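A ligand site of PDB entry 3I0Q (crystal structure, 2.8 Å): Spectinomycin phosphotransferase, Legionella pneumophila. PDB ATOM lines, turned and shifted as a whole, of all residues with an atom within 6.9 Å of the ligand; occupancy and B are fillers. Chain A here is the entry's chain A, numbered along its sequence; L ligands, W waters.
OD2 of Asp 230 sits close to OD2 of Asp 232 (2.6 Å).
O of Tyr 100 lies within hydrogen-bond range of N of Phe 50, at 2.6 Å.
The backbone NH (N) of Ile 229 sits at hydrogen-bond distance from the backbone carbonyl oxygen (O) of Asn 217, 2.8 Å away.
Merely in contact with the ligand: Ile 229, Phe 50, Asn 107, Phe 102, Ile 78, Leu 219, Tyr 100 and Gly 216.
Hydrophobic or aromatic side chains that line the ligand: Phe 50, Ile 78, Tyr 100, Phe 102, Ile 103, Leu 219 and Ile 229.
A nitrogen (N3) of the ligand sits at hydrogen-bond distance from the backbone carbonyl oxygen (O) of Pro 101 (3.2 Å).
An oxygen (O3) of the ligand lies within salt-bridge range of the side-chain amino group (NZ) of Lys 52 (3.7 Å).
The backbone NH of Ile 103 lies within hydrogen-bond range of a nitrogen (N4) of the ligand (3.0 Å).
The side-chain carboxylate (OD2) of Asp 230 lies close to an oxygen (O1) of the ligand (2.9 Å).
Water W2 bridges an oxygen (O7) of the ligand (2.5 Å) and the backbone carbonyl oxygen (O) of Ala 105 (3.1 Å).
Water W1 lies within hydrogen-bond range of OD1 of Asn 217 (2.7 Å), O1 of the ligand (3.1 Å) and OD1 of Asp 230 (3.4 Å).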
ATOM      1  N   ILE A  29     -21.843 -25.777   5.693  1.00  0.00           N
ATOM      2  CA  ILE A  29     -23.235 -25.515   5.343  1.00  0.00           C
ATOM      3  C   ILE A  29     -23.388 -24.094   4.796  1.00  0.00           C
ATOM      4  O   ILE A  29     -23.505 -23.136   5.567  1.00  0.00           O
ATOM      5  CB  ILE A  29     -24.136 -25.707   6.546  1.00  0.00           C
ATOM      6  CG1 ILE A  29     -23.893 -27.075   7.171  1.00  0.00           C
ATOM      7  CG2 ILE A  29     -25.577 -25.604   6.125  1.00  0.00           C
ATOM      8  CD1 ILE A  29     -24.639 -27.324   8.475  1.00  0.00           C
ATOM      9  N   ALA A  39     -20.905 -22.032   9.751  1.00  0.00           N
ATOM     10  CA  ALA A  39     -21.384 -23.207  10.462  1.00  0.00           C
ATOM     11  C   ALA A  39     -21.054 -24.468   9.666  1.00  0.00           C
ATOM     12  O   ALA A  39     -20.894 -24.392   8.450  1.00  0.00           O
ATOM     13  CB  ALA A  39     -22.871 -23.116  10.656  1.00  0.00           C
ATOM     14  N   TYR A  49     -22.735 -33.196  15.024  1.00  0.00           N
ATOM     15  CA  TYR A  49     -22.721 -31.894  15.671  1.00  0.00           C
ATOM     16  C   TYR A  49     -22.978 -30.728  14.696  1.00  0.00           C
ATOM     17  O   TYR A  49     -22.873 -30.880  13.470  1.00  0.00           O
ATOM     18  CB  TYR A  49     -21.376 -31.663  16.354  1.00  0.00           C
ATOM     19  CG  TYR A  49     -21.024 -32.685  17.385  1.00  0.00           C
ATOM     20  CD1 TYR A  49     -20.967 -32.365  18.746  1.00  0.00           C
ATOM     21  CD2 TYR A  49     -20.679 -33.995  17.001  1.00  0.00           C
ATOM     22  CE1 TYR A  49     -20.545 -33.312  19.701  1.00  0.00           C
ATOM     23  CE2 TYR A  49     -20.271 -34.957  17.942  1.00  0.00           C
ATOM     24  CZ  TYR A  49     -20.195 -34.604  19.284  1.00  0.00           C
ATOM     25  OH  TYR A  49     -19.704 -35.538  20.196  1.00  0.00           O
ATOM     26  N   PHE A  50     -23.313 -29.575  15.251  1.00  0.00           N
ATOM     27  CA  PHE A  50     -23.559 -28.368  14.494  1.00  0.00           C
ATOM     28  C   PHE A  50     -22.659 -27.346  15.165  1.00  0.00           C
ATOM     29  O   PHE A  50     -22.851 -27.026  16.335  1.00  0.00           O
ATOM     30  CB  PHE A  50     -25.047 -28.014  14.606  1.00  0.00           C
ATOM     31  CG  PHE A  50     -25.405 -26.682  14.008  1.00  0.00           C
ATOM     32  CD1 PHE A  50     -25.252 -25.510  14.735  1.00  0.00           C
ATOM     33  CD2 PHE A  50     -25.907 -26.596  12.719  1.00  0.00           C
ATOM     34  CE1 PHE A  50     -25.581 -24.273  14.183  1.00  0.00           C
ATOM     35  CE2 PHE A  50     -26.235 -25.350  12.162  1.00  0.00           C
ATOM     36  CZ  PHE A  50     -26.069 -24.191  12.890  1.00  0.00           C
ATOM     37  N   LYS A  52     -20.411 -23.470  15.176  1.00  0.00           N
ATOM     38  CA  LYS A  52     -20.581 -22.089  14.706  1.00  0.00           C
ATOM     39  C   LYS A  52     -19.314 -21.265  14.881  1.00  0.00           C
ATOM     40  O   LYS A  52     -18.963 -20.904  15.999  1.00  0.00           O
ATOM     41  CB  LYS A  52     -21.704 -21.370  15.462  1.00  0.00           C
ATOM     42  CG  LYS A  52     -23.112 -21.857  15.220  1.00  0.00           C
ATOM     43  CD  LYS A  52     -24.089 -21.043  16.090  1.00  0.00           C
ATOM     44  CE  LYS A  52     -25.534 -21.522  15.952  1.00  0.00           C
ATOM     45  NZ  LYS A  52     -26.493 -20.677  16.725  1.00  0.00           N
ATOM     46  N   LYS A  54     -17.665 -17.831  14.655  1.00  0.00           N
ATOM     47  CA  LYS A  54     -18.099 -16.440  14.550  1.00  0.00           C
ATOM     48  C   LYS A  54     -16.924 -15.476  14.682  1.00  0.00           C
ATOM     49  O   LYS A  54     -16.334 -15.371  15.764  1.00  0.00           O
ATOM     50  CB  LYS A  54     -19.142 -16.125  15.618  1.00  0.00           C
ATOM     51  CG  LYS A  54     -20.406 -16.983  15.567  1.00  0.00           C
ATOM     52  CD  LYS A  54     -21.478 -16.466  16.531  1.00  0.00           C
ATOM     53  CE  LYS A  54     -22.851 -17.046  16.221  1.00  0.00           C
ATOM     54  NZ  LYS A  54     -23.981 -16.412  16.981  1.00  0.00           N
ATOM     55  N   ILE A  78     -32.000 -25.658  22.353  1.00  0.00           N
ATOM     56  CA  ILE A  78     -30.813 -26.451  22.068  1.00  0.00           C
ATOM     57  C   ILE A  78     -29.635 -25.925  22.899  1.00  0.00           C
ATOM     58  O   ILE A  78     -29.268 -24.764  22.777  1.00  0.00           O
ATOM     59  CB  ILE A  78     -30.484 -26.405  20.556  1.00  0.00           C
ATOM     60  CG1 ILE A  78     -31.733 -26.766  19.745  1.00  0.00           C
ATOM     61  CG2 ILE A  78     -29.372 -27.393  20.230  1.00  0.00           C
ATOM     62  CD1 ILE A  78     -31.597 -26.612  18.251  1.00  0.00           C
ATOM     63  N   TYR A 100     -22.933 -27.486  19.008  1.00  0.00           N
ATOM     64  CA  TYR A 100     -24.291 -27.843  19.413  1.00  0.00           C
ATOM     65  C   TYR A 100     -24.501 -29.191  18.814  1.00  0.00           C
ATOM     66  O   TYR A 100     -23.922 -29.505  17.773  1.00  0.00           O
ATOM     67  CB  TYR A 100     -25.367 -26.939  18.809  1.00  0.00           C
ATOM     68  CG  TYR A 100     -25.374 -25.494  19.246  1.00  0.00           C
ATOM     69  CD1 TYR A 100     -24.676 -24.527  18.526  1.00  0.00           C
ATOM     70  CD2 TYR A 100     -26.106 -25.078  20.358  1.00  0.00           C
ATOM     71  CE1 TYR A 100     -24.710 -23.193  18.906  1.00  0.00           C
ATOM     72  CE2 TYR A 100     -26.153 -23.741  20.740  1.00  0.00           C
ATOM     73  CZ  TYR A 100     -25.448 -22.800  20.013  1.00  0.00           C
ATOM     74  OH  TYR A 100     -25.411 -21.479  20.391  1.00  0.00           O
ATOM     75  N   PRO A 101     -25.308 -30.029  19.461  1.00  0.00           N
ATOM     76  CA  PRO A 101     -25.546 -31.348  18.868  1.00  0.00           C
ATOM     77  C   PRO A 101     -26.328 -31.073  17.574  1.00  0.00           C
ATOM     78  O   PRO A 101     -26.915 -29.991  17.443  1.00  0.00           O
ATOM     79  CB  PRO A 101     -26.373 -32.058  19.938  1.00  0.00           C
ATOM     80  CG  PRO A 101     -27.165 -30.903  20.549  1.00  0.00           C
ATOM     81  CD  PRO A 101     -26.113 -29.832  20.676  1.00  0.00           C
ATOM     82  N   PHE A 102     -26.367 -31.998  16.624  1.00  0.00           N
ATOM     83  CA  PHE A 102     -27.078 -31.699  15.386  1.00  0.00           C
ATOM     84  C   PHE A 102     -28.520 -32.147  15.362  1.00  0.00           C
ATOM     85  O   PHE A 102     -28.798 -33.338  15.452  1.00  0.00           O
ATOM     86  CB  PHE A 102     -26.351 -32.274  14.166  1.00  0.00           C
ATOM     87  CG  PHE A 102     -26.750 -31.620  12.869  1.00  0.00           C
ATOM     88  CD1 PHE A 102     -26.028 -30.543  12.375  1.00  0.00           C
ATOM     89  CD2 PHE A 102     -27.889 -32.023  12.175  1.00  0.00           C
ATOM     90  CE1 PHE A 102     -26.434 -29.881  11.212  1.00  0.00           C
ATOM     91  CE2 PHE A 102     -28.296 -31.362  11.013  1.00  0.00           C
ATOM     92  CZ  PHE A 102     -27.562 -30.288  10.540  1.00  0.00           C
ATOM     93  N   ILE A 103     -29.432 -31.194  15.195  1.00  0.00           N
ATOM     94  CA  ILE A 103     -30.861 -31.512  15.146  1.00  0.00           C
ATOM     95  C   ILE A 103     -31.375 -31.628  13.726  1.00  0.00           C
ATOM     96  O   ILE A 103     -31.619 -30.624  13.058  1.00  0.00           O
ATOM     97  CB  ILE A 103     -31.703 -30.462  15.902  1.00  0.00           C
ATOM     98  CG1 ILE A 103     -31.655 -30.736  17.395  1.00  0.00           C
ATOM     99  CG2 ILE A 103     -33.158 -30.535  15.453  1.00  0.00           C
ATOM    100  CD1 ILE A 103     -30.258 -31.025  17.904  1.00  0.00           C
ATOM    101  N   HIS A 104     -31.531 -32.861  13.279  1.00  0.00           N
ATOM    102  CA  HIS A 104     -32.040 -33.162  11.941  1.00  0.00           C
ATOM    103  C   HIS A 104     -33.514 -32.836  11.972  1.00  0.00           C
ATOM    104  O   HIS A 104     -34.350 -33.670  12.301  1.00  0.00           O
ATOM    105  CB  HIS A 104     -31.859 -34.644  11.630  1.00  0.00           C
ATOM    106  CG  HIS A 104     -30.456 -35.125  11.770  1.00  0.00           C
ATOM    107  ND1 HIS A 104     -29.485 -34.873  10.823  1.00  0.00           N
ATOM    108  CD2 HIS A 104     -29.845 -35.851  12.743  1.00  0.00           C
ATOM    109  CE1 HIS A 104     -28.340 -35.422  11.207  1.00  0.00           C
ATOM    110  NE2 HIS A 104     -28.536 -36.018  12.366  1.00  0.00           N
ATOM    111  N   ALA A 105     -33.846 -31.604  11.629  1.00  0.00           N
ATOM    112  CA  ALA A 105     -35.243 -31.223  11.638  1.00  0.00           C
ATOM    113  C   ALA A 105     -35.452 -29.932  10.883  1.00  0.00           C
ATOM    114  O   ALA A 105     -34.665 -28.980  10.991  1.00  0.00           O
ATOM    115  CB  ALA A 105     -35.738 -31.069  13.067  1.00  0.00           C
ATOM    116  N   PRO A 106     -36.498 -29.891  10.077  1.00  0.00           N
ATOM    117  CA  PRO A 106     -36.842 -28.710   9.274  1.00  0.00           C
ATOM    118  C   PRO A 106     -37.482 -27.668  10.184  1.00  0.00           C
ATOM    119  O   PRO A 106     -37.803 -27.959  11.331  1.00  0.00           O
ATOM    120  CB  PRO A 106     -37.822 -29.274   8.261  1.00  0.00           C
ATOM    121  CG  PRO A 106     -38.562 -30.332   9.110  1.00  0.00           C
ATOM    122  CD  PRO A 106     -37.437 -31.010   9.838  1.00  0.00           C
ATOM    123  N   ASN A 107     -37.683 -26.456   9.672  1.00  0.00           N
ATOM    124  CA  ASN A 107     -38.307 -25.388  10.448  1.00  0.00           C
ATOM    125  C   ASN A 107     -39.753 -25.168  10.037  1.00  0.00           C
ATOM    126  O   ASN A 107     -40.278 -25.860   9.179  1.00  0.00           O
ATOM    127  CB  ASN A 107     -37.520 -24.070  10.313  1.00  0.00           C
ATOM    128  CG  ASN A 107     -37.327 -23.632   8.877  1.00  0.00           C
ATOM    129  OD1 ASN A 107     -38.198 -23.853   8.025  1.00  0.00           O
ATOM    130  ND2 ASN A 107     -36.201 -22.994   8.615  1.00  0.00           N
ATOM    131  N   GLY A 216     -39.516 -19.477  10.961  1.00  0.00           N
ATOM    132  CA  GLY A 216     -38.117 -19.712  10.638  1.00  0.00           C
ATOM    133  C   GLY A 216     -37.246 -20.090  11.810  1.00  0.00           C
ATOM    134  O   GLY A 216     -36.215 -20.741  11.636  1.00  0.00           O
ATOM    135  N   ASN A 217     -37.638 -19.709  13.019  1.00  0.00           N
ATOM    136  CA  ASN A 217     -36.821 -20.051  14.178  1.00  0.00           C
ATOM    137  C   ASN A 217     -37.312 -21.128  15.099  1.00  0.00           C
ATOM    138  O   ASN A 217     -36.856 -21.217  16.246  1.00  0.00           O
ATOM    139  CB  ASN A 217     -36.472 -18.801  14.955  1.00  0.00           C
ATOM    140  CG  ASN A 217     -35.523 -17.958  14.198  1.00  0.00           C
ATOM    141  OD1 ASN A 217     -34.571 -18.463  13.608  1.00  0.00           O
ATOM    142  ND2 ASN A 217     -35.756 -16.653  14.198  1.00  0.00           N
ATOM    143  N   VAL A 218     -38.210 -21.963  14.598  1.00  0.00           N
ATOM    144  CA  VAL A 218     -38.705 -23.093  15.352  1.00  0.00           C
ATOM    145  C   VAL A 218     -38.388 -24.347  14.518  1.00  0.00           C
ATOM    146  O   VAL A 218     -38.996 -24.569  13.464  1.00  0.00           O
ATOM    147  CB  VAL A 218     -40.256 -23.060  15.565  1.00  0.00           C
ATOM    148  CG1 VAL A 218     -40.656 -24.230  16.464  1.00  0.00           C
ATOM    149  CG2 VAL A 218     -40.699 -21.749  16.186  1.00  0.00           C
ATOM    150  N   LEU A 219     -37.424 -25.133  14.974  1.00  0.00           N
ATOM    151  CA  LEU A 219     -37.102 -26.374  14.292  1.00  0.00           C
ATOM    152  C   LEU A 219     -38.220 -27.291  14.727  1.00  0.00           C
ATOM    153  O   LEU A 219     -38.317 -27.614  15.912  1.00  0.00           O
ATOM    154  CB  LEU A 219     -35.779 -26.952  14.775  1.00  0.00           C
ATOM    155  CG  LEU A 219     -34.507 -26.163  14.557  1.00  0.00           C
ATOM    156  CD1 LEU A 219     -33.337 -27.086  14.813  1.00  0.00           C
ATOM    157  CD2 LEU A 219     -34.437 -25.628  13.120  1.00  0.00           C
ATOM    158  N   ILE A 229     -35.010 -21.375  18.308  1.00  0.00           N
ATOM    159  CA  ILE A 229     -33.616 -21.001  18.124  1.00  0.00           C
ATOM    160  C   ILE A 229     -33.298 -19.533  17.878  1.00  0.00           C
ATOM    161  O   ILE A 229     -34.144 -18.675  18.037  1.00  0.00           O
ATOM    162  CB  ILE A 229     -32.979 -21.829  17.001  1.00  0.00           C
ATOM    163  CG1 ILE A 229     -33.517 -21.393  15.637  1.00  0.00           C
ATOM    164  CG2 ILE A 229     -33.245 -23.311  17.260  1.00  0.00           C
ATOM    165  CD1 ILE A 229     -32.891 -22.158  14.525  1.00  0.00           C
ATOM    166  N   ASP A 230     -32.062 -19.266  17.500  1.00  0.00           N
ATOM    167  CA  ASP A 230     -31.598 -17.898  17.256  1.00  0.00           C
ATOM    168  C   ASP A 230     -31.934 -17.001  18.446  1.00  0.00           C
ATOM    169  O   ASP A 230     -32.961 -16.322  18.465  1.00  0.00           O
ATOM    170  CB  ASP A 230     -32.209 -17.291  15.973  1.00  0.00           C
ATOM    171  CG  ASP A 230     -31.183 -16.453  15.162  1.00  0.00           C
ATOM    172  OD1 ASP A 230     -31.587 -15.624  14.297  1.00  0.00           O
ATOM    173  OD2 ASP A 230     -29.961 -16.659  15.376  1.00  0.00           O
ATOM    174  N   TRP A 231     -31.075 -17.007  19.456  1.00  0.00           N
ATOM    175  CA  TRP A 231     -31.289 -16.151  20.601  1.00  0.00           C
ATOM    176  C   TRP A 231     -30.234 -15.079  20.560  1.00  0.00           C
ATOM    177  O   TRP A 231     -29.665 -14.703  21.595  1.00  0.00           O
ATOM    178  CB  TRP A 231     -31.209 -16.925  21.911  1.00  0.00           C
ATOM    179  CG  TRP A 231     -32.376 -17.832  22.104  1.00  0.00           C
ATOM    180  CD1 TRP A 231     -32.455 -19.142  21.759  1.00  0.00           C
ATOM    181  CD2 TRP A 231     -33.648 -17.470  22.629  1.00  0.00           C
ATOM    182  NE1 TRP A 231     -33.705 -19.632  22.032  1.00  0.00           N
ATOM    183  CE2 TRP A 231     -34.460 -18.625  22.579  1.00  0.00           C
ATOM    184  CE3 TRP A 231     -34.194 -16.299  23.148  1.00  0.00           C
ATOM    185  CZ2 TRP A 231     -35.786 -18.628  23.015  1.00  0.00           C
ATOM    186  CZ3 TRP A 231     -35.512 -16.302  23.589  1.00  0.00           C
ATOM    187  CH2 TRP A 231     -36.293 -17.467  23.525  1.00  0.00           C
ATOM    188  N   ASP A 232     -29.970 -14.573  19.376  1.00  0.00           N
ATOM    189  CA  ASP A 232     -28.973 -13.543  19.219  1.00  0.00           C
ATOM    190  C   ASP A 232     -29.436 -12.204  19.747  1.00  0.00           C
ATOM    191  O   ASP A 232     -28.659 -11.479  20.378  1.00  0.00           O
ATOM    192  CB  ASP A 232     -28.547 -13.416  17.747  1.00  0.00           C
ATOM    193  CG  ASP A 232     -27.694 -14.585  17.297  1.00  0.00           C
ATOM    194  OD1 ASP A 232     -26.681 -14.877  17.977  1.00  0.00           O
ATOM    195  OD2 ASP A 232     -28.038 -15.217  16.270  1.00  0.00           O
HETATM  196  P1  LIG L   1     -29.536 -19.662  13.543  1.00  0.00           P
HETATM  197  O1  LIG L   1     -29.681 -18.290  12.990  1.00  0.00           O
HETATM  198  O2  LIG L   1     -28.114 -20.267  13.076  1.00  0.00           O
HETATM  199  O3  LIG L   1     -29.665 -19.883  15.015  1.00  0.00           O
HETATM  200  O4  LIG L   1     -30.584 -20.635  12.780  1.00  0.00           O
HETATM  201  C1  LIG L   1     -30.738 -20.583  11.347  1.00  0.00           C
HETATM  202  C2  LIG L   1     -30.798 -21.996  10.759  1.00  0.00           C
HETATM  203  O5  LIG L   1     -29.701 -22.795  11.187  1.00  0.00           O
HETATM  204  C3  LIG L   1     -32.025 -22.805  11.145  1.00  0.00           C
HETATM  205  O6  LIG L   1     -33.045 -22.623  10.147  1.00  0.00           O
HETATM  206  C4  LIG L   1     -31.492 -24.255  11.084  1.00  0.00           C
HETATM  207  O7  LIG L   1     -31.632 -24.725   9.729  1.00  0.00           O
HETATM  208  C5  LIG L   1     -29.995 -24.185  11.418  1.00  0.00           C
HETATM  209  N1  LIG L   1     -29.594 -24.682  12.770  1.00  0.00           N
HETATM  210  C6  LIG L   1     -29.384 -23.941  13.914  1.00  0.00           C
HETATM  211  N2  LIG L   1     -29.034 -24.636  14.957  1.00  0.00           N
HETATM  212  C7  LIG L   1     -29.011 -25.941  14.490  1.00  0.00           C
HETATM  213  C8  LIG L   1     -28.710 -27.205  15.118  1.00  0.00           C
HETATM  214  N3  LIG L   1     -28.378 -27.309  16.405  1.00  0.00           N
HETATM  215  N4  LIG L   1     -28.788 -28.340  14.352  1.00  0.00           N
HETATM  216  C9  LIG L   1     -29.127 -28.229  13.056  1.00  0.00           C
HETATM  217  N5  LIG L   1     -29.430 -27.110  12.352  1.00  0.00           N
HETATM  218  C10 LIG L   1     -29.349 -25.991  13.156  1.00  0.00           C
HETATM  219  O   HOH W   1     -32.563 -17.819  11.922  1.00  0.00           O
HETATM  220  O   HOH W   2     -32.791 -26.939   9.666  1.00  0.00           O
